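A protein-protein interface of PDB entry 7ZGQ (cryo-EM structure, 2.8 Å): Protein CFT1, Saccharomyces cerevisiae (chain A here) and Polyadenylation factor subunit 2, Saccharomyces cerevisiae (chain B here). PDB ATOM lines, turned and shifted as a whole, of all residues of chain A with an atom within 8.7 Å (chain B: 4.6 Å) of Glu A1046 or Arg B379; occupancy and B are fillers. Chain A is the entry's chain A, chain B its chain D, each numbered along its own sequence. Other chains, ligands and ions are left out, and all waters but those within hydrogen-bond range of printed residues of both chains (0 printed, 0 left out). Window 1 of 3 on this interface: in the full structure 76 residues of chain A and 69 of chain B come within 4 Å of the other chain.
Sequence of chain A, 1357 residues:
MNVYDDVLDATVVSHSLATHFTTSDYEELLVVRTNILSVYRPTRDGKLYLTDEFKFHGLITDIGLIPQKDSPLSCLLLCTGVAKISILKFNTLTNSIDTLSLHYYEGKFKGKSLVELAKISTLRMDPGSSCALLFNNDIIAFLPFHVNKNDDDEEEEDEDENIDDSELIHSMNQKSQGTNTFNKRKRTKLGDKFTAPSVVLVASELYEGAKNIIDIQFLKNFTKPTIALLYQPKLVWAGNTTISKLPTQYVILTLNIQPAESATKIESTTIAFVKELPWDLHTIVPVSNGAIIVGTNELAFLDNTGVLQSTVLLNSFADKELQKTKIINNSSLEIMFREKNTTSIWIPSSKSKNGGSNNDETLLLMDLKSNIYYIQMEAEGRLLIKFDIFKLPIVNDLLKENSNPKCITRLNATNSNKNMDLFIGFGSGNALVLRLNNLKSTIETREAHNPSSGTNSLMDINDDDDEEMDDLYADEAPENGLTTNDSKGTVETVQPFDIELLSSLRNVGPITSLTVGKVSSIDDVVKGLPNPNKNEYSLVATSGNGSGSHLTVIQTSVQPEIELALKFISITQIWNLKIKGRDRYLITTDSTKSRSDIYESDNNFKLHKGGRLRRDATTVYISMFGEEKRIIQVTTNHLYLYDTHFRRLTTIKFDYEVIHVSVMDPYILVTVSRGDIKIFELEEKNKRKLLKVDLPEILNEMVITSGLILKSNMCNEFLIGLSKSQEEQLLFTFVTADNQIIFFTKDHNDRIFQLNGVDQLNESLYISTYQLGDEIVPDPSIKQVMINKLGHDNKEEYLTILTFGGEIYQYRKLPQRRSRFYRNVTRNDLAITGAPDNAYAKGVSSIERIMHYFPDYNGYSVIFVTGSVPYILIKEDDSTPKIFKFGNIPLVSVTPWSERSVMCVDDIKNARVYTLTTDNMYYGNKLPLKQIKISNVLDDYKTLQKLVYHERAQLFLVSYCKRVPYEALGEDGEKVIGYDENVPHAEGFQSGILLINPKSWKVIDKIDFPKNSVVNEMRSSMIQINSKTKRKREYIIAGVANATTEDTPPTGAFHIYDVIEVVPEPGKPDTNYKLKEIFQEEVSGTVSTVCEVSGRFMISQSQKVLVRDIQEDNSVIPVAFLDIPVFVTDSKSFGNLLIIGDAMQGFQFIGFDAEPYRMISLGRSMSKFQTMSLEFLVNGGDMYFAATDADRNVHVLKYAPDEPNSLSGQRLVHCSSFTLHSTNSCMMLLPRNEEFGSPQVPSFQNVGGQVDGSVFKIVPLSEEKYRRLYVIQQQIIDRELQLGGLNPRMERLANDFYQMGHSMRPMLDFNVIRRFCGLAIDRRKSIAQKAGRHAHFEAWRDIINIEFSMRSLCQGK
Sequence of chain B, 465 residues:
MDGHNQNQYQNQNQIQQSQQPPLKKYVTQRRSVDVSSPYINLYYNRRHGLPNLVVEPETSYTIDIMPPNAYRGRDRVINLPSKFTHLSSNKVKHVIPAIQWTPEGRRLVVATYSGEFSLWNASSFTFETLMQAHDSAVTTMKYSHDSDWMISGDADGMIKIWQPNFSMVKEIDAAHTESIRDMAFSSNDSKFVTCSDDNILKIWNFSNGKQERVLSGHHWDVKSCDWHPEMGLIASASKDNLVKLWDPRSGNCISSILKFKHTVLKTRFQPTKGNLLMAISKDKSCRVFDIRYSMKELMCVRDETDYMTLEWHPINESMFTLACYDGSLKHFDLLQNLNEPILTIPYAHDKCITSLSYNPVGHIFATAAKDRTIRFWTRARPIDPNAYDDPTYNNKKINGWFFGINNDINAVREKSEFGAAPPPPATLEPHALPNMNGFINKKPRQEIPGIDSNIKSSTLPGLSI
NH2 of Arg B379 lies within salt-bridge range of OE2 of Glu A1046 (3.7 Å).
OD2 of Asp A1047 is in salt-bridge range of NE of Arg B381 (3.9 Å).
O of Glu A1046 sits close to O of Ser B32, 3.4 Å away.
O of Met B66 sits at hydrogen-bond distance from NH1 of Arg B379 (2.7 Å).
Ile B65 touches Trp A237.
Trp A237 touches Ala B380 (CH2 to O, 3.1 Å).
CA of Gly A239 touches O of Arg B381, 3.7 Å away.
Glu A1046 touches Val B33.
Glu A1046 touches Asp B34 (CG to O, 3.1 Å).
OE2 of Glu A1046 touches CG2 of Val B35, at 3.7 Å.
Pro B38 touches Glu A1046 (CG to CB, 3.7 Å).
His B363 touches Glu A1046.
OG of Ser B32 touches CA of Pro A1049 (3.5 Å).
Pro A1050 touches Asp B34 (CG to OD2, 3.2 Å).
Printed residues of chain B within 4 Å of Gly A239: Arg B381 (3.7 Å).
Glu A1046 touches just these residues of chain B: Ser B32 (3.4 Å), Val B33 (3.6 Å), Asp B34 (3.1 Å), Val B35 (3.7 Å), Pro B38 (3.7 Å), His B363 (3.7 Å) and Arg B379 (3.7 Å).
Printed residues of chain A within 4 Å of Pro B38: Glu A1046 (3.7 Å).
Printed residues of chain A within 4 Å of Ile B78: Trp A237.
No residue of chain A comes within 4 Å of Thr B378.
Arg B379 touches just one residue of chain A: Glu A1046.
Of chain A, only Trp A237 comes within 4 Å of Ala B380.
Of the printed residues of chain A, Arg B381 touches Gly A239 (3.7 Å) and Asp A1047 (3.5 Å).
The nearest residue of chain A that does not touch Arg B379 is Trp A237 (5.6 Å).
Hydrophobic or aromatic side chains of chain A that line the printed part of chain B: Trp A237, Pro A1049 and Pro A1050.
Hydrophobic or aromatic side chains of chain B within 4 Å of the printed part of chain A: Val B35, Pro B38, Ile B65, Ile B78, His B363 and Ala B380.
Among the printed residues, Asp or Glu carboxylates within 4 Å of a Lys or Arg side-chain nitrogen of the other chain: Glu A1046 with Arg B379 and Asp A1047 with Arg B381.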
ATOM      1  N   TRP A 237       1.829 -17.773  19.385  1.00  0.00           N
ATOM      2  CA  TRP A 237       3.078 -18.356  19.851  1.00  0.00           C
ATOM      3  C   TRP A 237       2.818 -19.051  21.188  1.00  0.00           C
ATOM      4  O   TRP A 237       1.670 -19.216  21.608  1.00  0.00           O
ATOM      5  CB  TRP A 237       4.174 -17.292  19.944  1.00  0.00           C
ATOM      6  CG  TRP A 237       4.109 -16.434  21.167  1.00  0.00           C
ATOM      7  CD1 TRP A 237       3.172 -15.488  21.455  1.00  0.00           C
ATOM      8  CD2 TRP A 237       5.031 -16.431  22.262  1.00  0.00           C
ATOM      9  NE1 TRP A 237       3.448 -14.901  22.666  1.00  0.00           N
ATOM     10  CE2 TRP A 237       4.585 -15.463  23.181  1.00  0.00           C
ATOM     11  CE3 TRP A 237       6.188 -17.158  22.557  1.00  0.00           C
ATOM     12  CZ2 TRP A 237       5.256 -15.202  24.373  1.00  0.00           C
ATOM     13  CZ3 TRP A 237       6.852 -16.897  23.740  1.00  0.00           C
ATOM     14  CH2 TRP A 237       6.385 -15.928  24.633  1.00  0.00           C
ATOM     15  N   GLY A 239       2.980 -18.110  24.087  1.00  0.00           N
ATOM     16  CA  GLY A 239       2.263 -17.317  25.066  1.00  0.00           C
ATOM     17  C   GLY A 239       0.828 -17.027  24.677  1.00  0.00           C
ATOM     18  O   GLY A 239       0.022 -16.612  25.515  1.00  0.00           O
ATOM     19  N   TYR A 966      18.515 -26.479  30.829  1.00  0.00           N
ATOM     20  CA  TYR A 966      18.503 -25.241  31.595  1.00  0.00           C
ATOM     21  C   TYR A 966      17.405 -25.285  32.648  1.00  0.00           C
ATOM     22  O   TYR A 966      16.256 -25.625  32.343  1.00  0.00           O
ATOM     23  CB  TYR A 966      18.300 -24.031  30.682  1.00  0.00           C
ATOM     24  CG  TYR A 966      17.999 -22.754  31.431  1.00  0.00           C
ATOM     25  CD1 TYR A 966      18.945 -22.181  32.269  1.00  0.00           C
ATOM     26  CD2 TYR A 966      16.770 -22.124  31.304  1.00  0.00           C
ATOM     27  CE1 TYR A 966      18.677 -21.015  32.957  1.00  0.00           C
ATOM     28  CE2 TYR A 966      16.492 -20.956  31.988  1.00  0.00           C
ATOM     29  CZ  TYR A 966      17.449 -20.407  32.814  1.00  0.00           C
ATOM     30  OH  TYR A 966      17.180 -19.245  33.498  1.00  0.00           O
ATOM     31  N   ALA A 968      15.484 -22.818  35.191  1.00  0.00           N
ATOM     32  CA  ALA A 968      15.245 -21.396  35.428  1.00  0.00           C
ATOM     33  C   ALA A 968      15.072 -21.166  36.923  1.00  0.00           C
ATOM     34  O   ALA A 968      14.005 -21.418  37.486  1.00  0.00           O
ATOM     35  CB  ALA A 968      14.028 -20.917  34.649  1.00  0.00           C
ATOM     36  N   ALA A1043      24.699 -17.373  31.432  1.00  0.00           N
ATOM     37  CA  ALA A1043      23.602 -17.344  30.468  1.00  0.00           C
ATOM     38  C   ALA A1043      22.321 -17.769  31.171  1.00  0.00           C
ATOM     39  O   ALA A1043      22.098 -18.954  31.424  1.00  0.00           O
ATOM     40  CB  ALA A1043      23.907 -18.246  29.278  1.00  0.00           C
ATOM     41  N   THR A1044      21.473 -16.793  31.489  1.00  0.00           N
ATOM     42  CA  THR A1044      20.201 -17.051  32.151  1.00  0.00           C
ATOM     43  C   THR A1044      19.063 -16.410  31.367  1.00  0.00           C
ATOM     44  O   THR A1044      19.255 -15.986  30.224  1.00  0.00           O
ATOM     45  CB  THR A1044      20.225 -16.533  33.590  1.00  0.00           C
ATOM     46  OG1 THR A1044      20.555 -15.138  33.592  1.00  0.00           O
ATOM     47  CG2 THR A1044      21.253 -17.292  34.416  1.00  0.00           C
ATOM     48  N   THR A1045      17.873 -16.352  31.957  1.00  0.00           N
ATOM     49  CA  THR A1045      16.732 -15.743  31.294  1.00  0.00           C
ATOM     50  C   THR A1045      16.729 -14.231  31.521  1.00  0.00           C
ATOM     51  O   THR A1045      17.590 -13.672  32.203  1.00  0.00           O
ATOM     52  CB  THR A1045      15.429 -16.377  31.777  1.00  0.00           C
ATOM     53  OG1 THR A1045      14.321 -15.739  31.131  1.00  0.00           O
ATOM     54  CG2 THR A1045      15.284 -16.226  33.280  1.00  0.00           C
ATOM     55  N   GLU A1046      15.741 -13.557  30.931  1.00  0.00           N
ATOM     56  CA  GLU A1046      15.625 -12.110  31.045  1.00  0.00           C
ATOM     57  C   GLU A1046      15.084 -11.667  32.400  1.00  0.00           C
ATOM     58  O   GLU A1046      15.199 -10.485  32.743  1.00  0.00           O
ATOM     59  CB  GLU A1046      14.725 -11.574  29.929  1.00  0.00           C
ATOM     60  CG  GLU A1046      14.842 -10.081  29.676  1.00  0.00           C
ATOM     61  CD  GLU A1046      13.849  -9.586  28.645  1.00  0.00           C
ATOM     62  OE1 GLU A1046      12.659  -9.950  28.742  1.00  0.00           O
ATOM     63  OE2 GLU A1046      14.261  -8.833  27.737  1.00  0.00           O
ATOM     64  N   ASP A1047      14.515 -12.582  33.179  1.00  0.00           N
ATOM     65  CA  ASP A1047      13.855 -12.247  34.433  1.00  0.00           C
ATOM     66  C   ASP A1047      14.792 -12.291  35.635  1.00  0.00           C
ATOM     67  O   ASP A1047      14.333 -12.117  36.767  1.00  0.00           O
ATOM     68  CB  ASP A1047      12.669 -13.185  34.666  1.00  0.00           C
ATOM     69  CG  ASP A1047      11.765 -13.289  33.454  1.00  0.00           C
ATOM     70  OD1 ASP A1047      11.709 -12.320  32.668  1.00  0.00           O
ATOM     71  OD2 ASP A1047      11.109 -14.338  33.286  1.00  0.00           O
ATOM     72  N   THR A1048      16.085 -12.518  35.420  1.00  0.00           N
ATOM     73  CA  THR A1048      17.051 -12.526  36.504  1.00  0.00           C
ATOM     74  C   THR A1048      18.146 -11.499  36.237  1.00  0.00           C
ATOM     75  O   THR A1048      18.517 -11.270  35.082  1.00  0.00           O
ATOM     76  CB  THR A1048      17.685 -13.912  36.676  1.00  0.00           C
ATOM     77  OG1 THR A1048      19.017 -13.772  37.185  1.00  0.00           O
ATOM     78  CG2 THR A1048      17.735 -14.634  35.348  1.00  0.00           C
ATOM     79  N   PRO A1049      18.670 -10.859  37.280  1.00  0.00           N
ATOM     80  CA  PRO A1049      19.725  -9.860  37.086  1.00  0.00           C
ATOM     81  C   PRO A1049      20.958 -10.479  36.456  1.00  0.00           C
ATOM     82  O   PRO A1049      21.336 -11.613  36.788  1.00  0.00           O
ATOM     83  CB  PRO A1049      20.014  -9.366  38.512  1.00  0.00           C
ATOM     84  CG  PRO A1049      19.515 -10.449  39.397  1.00  0.00           C
ATOM     85  CD  PRO A1049      18.321 -11.017  38.700  1.00  0.00           C
ATOM     86  N   PRO A1050      21.612  -9.766  35.544  1.00  0.00           N
ATOM     87  CA  PRO A1050      22.796 -10.324  34.885  1.00  0.00           C
ATOM     88  C   PRO A1050      23.975 -10.419  35.840  1.00  0.00           C
ATOM     89  O   PRO A1050      24.239  -9.506  36.625  1.00  0.00           O
ATOM     90  CB  PRO A1050      23.071  -9.330  33.752  1.00  0.00           C
ATOM     91  CG  PRO A1050      22.467  -8.055  34.221  1.00  0.00           C
ATOM     92  CD  PRO A1050      21.271  -8.425  35.041  1.00  0.00           C
ATOM     93  N   SER B  32      14.374  -7.583  38.159  1.00  0.00           N
ATOM     94  CA  SER B  32      15.271  -7.083  37.125  1.00  0.00           C
ATOM     95  C   SER B  32      14.812  -7.575  35.761  1.00  0.00           C
ATOM     96  O   SER B  32      14.516  -8.763  35.592  1.00  0.00           O
ATOM     97  CB  SER B  32      16.712  -7.526  37.387  1.00  0.00           C
ATOM     98  OG  SER B  32      17.522  -7.315  36.245  1.00  0.00           O
ATOM     99  N   VAL B  33      14.755  -6.662  34.795  1.00  0.00           N
ATOM    100  CA  VAL B  33      14.414  -6.988  33.409  1.00  0.00           C
ATOM    101  C   VAL B  33      15.551  -6.444  32.548  1.00  0.00           C
ATOM    102  O   VAL B  33      15.529  -5.285  32.121  1.00  0.00           O
ATOM    103  CB  VAL B  33      13.065  -6.403  32.978  1.00  0.00           C
ATOM    104  CG1 VAL B  33      12.676  -6.928  31.606  1.00  0.00           C
ATOM    105  CG2 VAL B  33      11.989  -6.728  34.001  1.00  0.00           C
ATOM    106  N   ASP B  34      16.552  -7.281  32.281  1.00  0.00           N
ATOM    107  CA  ASP B  34      17.703  -6.894  31.479  1.00  0.00           C
ATOM    108  C   ASP B  34      17.844  -7.831  30.289  1.00  0.00           C
ATOM    109  O   ASP B  34      17.713  -9.051  30.427  1.00  0.00           O
ATOM    110  CB  ASP B  34      18.991  -6.899  32.304  1.00  0.00           C
ATOM    111  CG  ASP B  34      20.028  -5.932  31.765  1.00  0.00           C
ATOM    112  OD1 ASP B  34      19.685  -5.130  30.871  1.00  0.00           O
ATOM    113  OD2 ASP B  34      21.184  -5.971  32.233  1.00  0.00           O
ATOM    114  N   VAL B  35      18.136  -7.252  29.127  1.00  0.00           N
ATOM    115  CA  VAL B  35      18.144  -7.978  27.863  1.00  0.00           C
ATOM    116  C   VAL B  35      19.540  -8.522  27.575  1.00  0.00           C
ATOM    117  O   VAL B  35      19.827  -8.980  26.463  1.00  0.00           O
ATOM    118  CB  VAL B  35      17.633  -7.067  26.727  1.00  0.00           C
ATOM    119  CG1 VAL B  35      18.728  -6.120  26.245  1.00  0.00           C
ATOM    120  CG2 VAL B  35      17.056  -7.889  25.583  1.00  0.00           C
ATOM    121  N   PRO B  38      19.540 -12.625  27.161  1.00  0.00           N
ATOM    122  CA  PRO B  38      18.928 -12.948  25.862  1.00  0.00           C
ATOM    123  C   PRO B  38      19.801 -12.567  24.682  1.00  0.00           C
ATOM    124  O   PRO B  38      19.826 -13.290  23.681  1.00  0.00           O
ATOM    125  CB  PRO B  38      17.620 -12.149  25.886  1.00  0.00           C
ATOM    126  CG  PRO B  38      17.280 -12.048  27.320  1.00  0.00           C
ATOM    127  CD  PRO B  38      18.585 -11.938  28.051  1.00  0.00           C
ATOM    128  N   ILE B  65      13.677 -17.266  24.517  1.00  0.00           N
ATOM    129  CA  ILE B  65      12.966 -16.074  24.065  1.00  0.00           C
ATOM    130  C   ILE B  65      14.009 -15.039  23.661  1.00  0.00           C
ATOM    131  O   ILE B  65      14.707 -14.481  24.513  1.00  0.00           O
ATOM    132  CB  ILE B  65      12.027 -15.529  25.144  1.00  0.00           C
ATOM    133  CG1 ILE B  65      10.910 -16.532  25.434  1.00  0.00           C
ATOM    134  CG2 ILE B  65      11.442 -14.194  24.708  1.00  0.00           C
ATOM    135  CD1 ILE B  65       9.791 -15.974  26.282  1.00  0.00           C
ATOM    136  N   MET B  66      14.126 -14.790  22.362  1.00  0.00           N
ATOM    137  CA  MET B  66      15.141 -13.886  21.861  1.00  0.00           C
ATOM    138  C   MET B  66      14.777 -12.443  22.192  1.00  0.00           C
ATOM    139  O   MET B  66      13.622 -12.138  22.497  1.00  0.00           O
ATOM    140  CB  MET B  66      15.304 -14.064  20.355  1.00  0.00           C
ATOM    141  CG  MET B  66      16.195 -15.229  19.974  1.00  0.00           C
ATOM    142  SD  MET B  66      17.555 -15.447  21.135  1.00  0.00           S
ATOM    143  CE  MET B  66      17.249 -17.110  21.717  1.00  0.00           C
ATOM    144  N   PRO B  67      15.754 -11.537  22.165  1.00  0.00           N
ATOM    145  CA  PRO B  67      15.436 -10.127  22.343  1.00  0.00           C
ATOM    146  C   PRO B  67      14.501  -9.653  21.250  1.00  0.00           C
ATOM    147  O   PRO B  67      14.498 -10.197  20.130  1.00  0.00           O
ATOM    148  CB  PRO B  67      16.808  -9.440  22.253  1.00  0.00           C
ATOM    149  CG  PRO B  67      17.741 -10.460  21.703  1.00  0.00           C
ATOM    150  CD  PRO B  67      17.205 -11.775  22.138  1.00  0.00           C
ATOM    151  N   PRO B  68      13.670  -8.648  21.536  1.00  0.00           N
ATOM    152  CA  PRO B  68      12.615  -8.270  20.581  1.00  0.00           C
ATOM    153  C   PRO B  68      13.124  -7.873  19.207  1.00  0.00           C
ATOM    154  O   PRO B  68      12.395  -8.037  18.221  1.00  0.00           O
ATOM    155  CB  PRO B  68      11.909  -7.097  21.280  1.00  0.00           C
ATOM    156  CG  PRO B  68      12.780  -6.719  22.432  1.00  0.00           C
ATOM    157  CD  PRO B  68      13.552  -7.927  22.811  1.00  0.00           C
ATOM    158  N   TYR B  71      13.135 -10.758  16.426  1.00  0.00           N
ATOM    159  CA  TYR B  71      11.901 -11.339  15.917  1.00  0.00           C
ATOM    160  C   TYR B  71      11.313 -10.453  14.828  1.00  0.00           C
ATOM    161  O   TYR B  71      11.184  -9.239  15.010  1.00  0.00           O
ATOM    162  CB  TYR B  71      10.888 -11.530  17.044  1.00  0.00           C
ATOM    163  CG  TYR B  71      11.271 -12.607  18.032  1.00  0.00           C
ATOM    164  CD1 TYR B  71      11.642 -13.871  17.600  1.00  0.00           C
ATOM    165  CD2 TYR B  71      11.263 -12.358  19.396  1.00  0.00           C
ATOM    166  CE1 TYR B  71      11.991 -14.859  18.499  1.00  0.00           C
ATOM    167  CE2 TYR B  71      11.612 -13.337  20.302  1.00  0.00           C
ATOM    168  CZ  TYR B  71      11.972 -14.585  19.849  1.00  0.00           C
ATOM    169  OH  TYR B  71      12.321 -15.563  20.751  1.00  0.00           O
ATOM    170  N   ILE B  78       5.379 -12.412  19.396  1.00  0.00           N
ATOM    171  CA  ILE B  78       6.100 -12.552  20.654  1.00  0.00           C
ATOM    172  C   ILE B  78       6.473 -11.196  21.237  1.00  0.00           C
ATOM    173  O   ILE B  78       6.736 -11.092  22.440  1.00  0.00           O
ATOM    174  CB  ILE B  78       7.353 -13.429  20.456  1.00  0.00           C
ATOM    175  CG1 ILE B  78       7.027 -14.626  19.564  1.00  0.00           C
ATOM    176  CG2 ILE B  78       7.891 -13.910  21.792  1.00  0.00           C
ATOM    177  CD1 ILE B  78       8.217 -15.516  19.284  1.00  0.00           C
ATOM    178  N   ASN B  79       6.487 -10.149  20.418  1.00  0.00           N
ATOM    179  CA  ASN B  79       6.844  -8.811  20.864  1.00  0.00           C
ATOM    180  C   ASN B  79       5.665  -8.051  21.457  1.00  0.00           C
ATOM    181  O   ASN B  79       5.822  -6.883  21.823  1.00  0.00           O
ATOM    182  CB  ASN B  79       7.438  -8.010  19.703  1.00  0.00           C
ATOM    183  CG  ASN B  79       8.838  -8.459  19.348  1.00  0.00           C
ATOM    184  OD1 ASN B  79       9.541  -9.040  20.172  1.00  0.00           O
ATOM    185  ND2 ASN B  79       9.250  -8.194  18.116  1.00  0.00           N
ATOM    186  N   LEU B  80       4.501  -8.678  21.550  1.00  0.00           N
ATOM    187  CA  LEU B  80       3.328  -8.009  22.095  1.00  0.00           C
ATOM    188  C   LEU B  80       3.527  -7.723  23.581  1.00  0.00           C
ATOM    189  O   LEU B  80       3.874  -8.635  24.341  1.00  0.00           O
ATOM    190  CB  LEU B  80       2.088  -8.875  21.886  1.00  0.00           C
ATOM    191  CG  LEU B  80       0.758  -8.164  21.636  1.00  0.00           C
ATOM    192  CD1 LEU B  80       0.936  -7.005  20.671  1.00  0.00           C
ATOM    193  CD2 LEU B  80      -0.269  -9.151  21.107  1.00  0.00           C
ATOM    194  N   LYS B  83       1.999  -8.544  29.111  1.00  0.00           N
ATOM    195  CA  LYS B  83       2.192  -8.812  30.528  1.00  0.00           C
ATOM    196  C   LYS B  83       2.371  -7.514  31.302  1.00  0.00           C
ATOM    197  O   LYS B  83       3.023  -6.580  30.830  1.00  0.00           O
ATOM    198  CB  LYS B  83       3.409  -9.713  30.739  1.00  0.00           C
ATOM    199  CG  LYS B  83       3.673 -10.080  32.188  1.00  0.00           C
ATOM    200  CD  LYS B  83       4.773 -11.120  32.302  1.00  0.00           C
ATOM    201  CE  LYS B  83       4.801 -11.744  33.686  1.00  0.00           C
ATOM    202  NZ  LYS B  83       5.639 -10.960  34.633  1.00  0.00           N
ATOM    203  N   HIS B 363      11.650  -4.281  24.725  1.00  0.00           N
ATOM    204  CA  HIS B 363      11.262  -5.291  25.698  1.00  0.00           C
ATOM    205  C   HIS B 363      10.359  -4.757  26.802  1.00  0.00           C
ATOM    206  O   HIS B 363       9.827  -5.557  27.579  1.00  0.00           O
ATOM    207  CB  HIS B 363      12.508  -5.927  26.324  1.00  0.00           C
ATOM    208  CG  HIS B 363      13.344  -4.974  27.121  1.00  0.00           C
ATOM    209  ND1 HIS B 363      13.738  -3.744  26.640  1.00  0.00           N
ATOM    210  CD2 HIS B 363      13.870  -5.075  28.365  1.00  0.00           C
ATOM    211  CE1 HIS B 363      14.464  -3.127  27.554  1.00  0.00           C
ATOM    212  NE2 HIS B 363      14.560  -3.914  28.609  1.00  0.00           N
ATOM    213  N   THR B 378       5.743  -5.810  29.756  1.00  0.00           N
ATOM    214  CA  THR B 378       6.770  -6.608  29.102  1.00  0.00           C
ATOM    215  C   THR B 378       6.113  -7.654  28.208  1.00  0.00           C
ATOM    216  O   THR B 378       4.889  -7.791  28.163  1.00  0.00           O
ATOM    217  CB  THR B 378       7.686  -7.274  30.133  1.00  0.00           C
ATOM    218  OG1 THR B 378       6.894  -7.837  31.187  1.00  0.00           O
ATOM    219  CG2 THR B 378       8.652  -6.261  30.718  1.00  0.00           C
ATOM    220  N   ARG B 379       6.949  -8.397  27.490  1.00  0.00           N
ATOM    221  CA  ARG B 379       6.455  -9.455  26.625  1.00  0.00           C
ATOM    222  C   ARG B 379       5.974 -10.642  27.455  1.00  0.00           C
ATOM    223  O   ARG B 379       6.383 -10.843  28.602  1.00  0.00           O
ATOM    224  CB  ARG B 379       7.541  -9.900  25.647  1.00  0.00           C
ATOM    225  CG  ARG B 379       7.935  -8.838  24.636  1.00  0.00           C
ATOM    226  CD  ARG B 379       9.112  -9.293  23.793  1.00  0.00           C
ATOM    227  NE  ARG B 379      10.302  -9.537  24.598  1.00  0.00           N
ATOM    228  CZ  ARG B 379      11.319 -10.297  24.217  1.00  0.00           C
ATOM    229  NH1 ARG B 379      11.324 -10.908  23.044  1.00  0.00           N
ATOM    230  NH2 ARG B 379      12.358 -10.448  25.034  1.00  0.00           N
ATOM    231  N   ALA B 380       5.090 -11.432  26.857  1.00  0.00           N
ATOM    232  CA  ALA B 380       4.524 -12.578  27.550  1.00  0.00           C
ATOM    233  C   ALA B 380       5.563 -13.683  27.716  1.00  0.00           C
ATOM    234  O   ALA B 380       6.515 -13.807  26.940  1.00  0.00           O
ATOM    235  CB  ALA B 380       3.306 -13.112  26.798  1.00  0.00           C
ATOM    236  N   ARG B 381       5.371 -14.485  28.751  1.00  0.00           N
ATOM    237  CA  ARG B 381       6.161 -15.667  29.047  1.00  0.00           C
ATOM    238  C   ARG B 381       5.493 -16.904  28.468  1.00  0.00           C
ATOM    239  O   ARG B 381       4.289 -16.897  28.193  1.00  0.00           O
ATOM    240  CB  ARG B 381       6.333 -15.820  30.563  1.00  0.00           C
ATOM    241  CG  ARG B 381       6.594 -14.509  31.290  1.00  0.00           C
ATOM    242  CD  ARG B 381       8.085 -14.253  31.465  1.00  0.00           C
ATOM    243  NE  ARG B 381       8.771 -14.071  30.191  1.00  0.00           N
ATOM    244  CZ  ARG B 381       8.737 -12.959  29.469  1.00  0.00           C
ATOM    245  NH1 ARG B 381       8.061 -11.895  29.870  1.00  0.00           N
ATOM    246  NH2 ARG B 381       9.399 -12.913  28.317  1.00  0.00           N
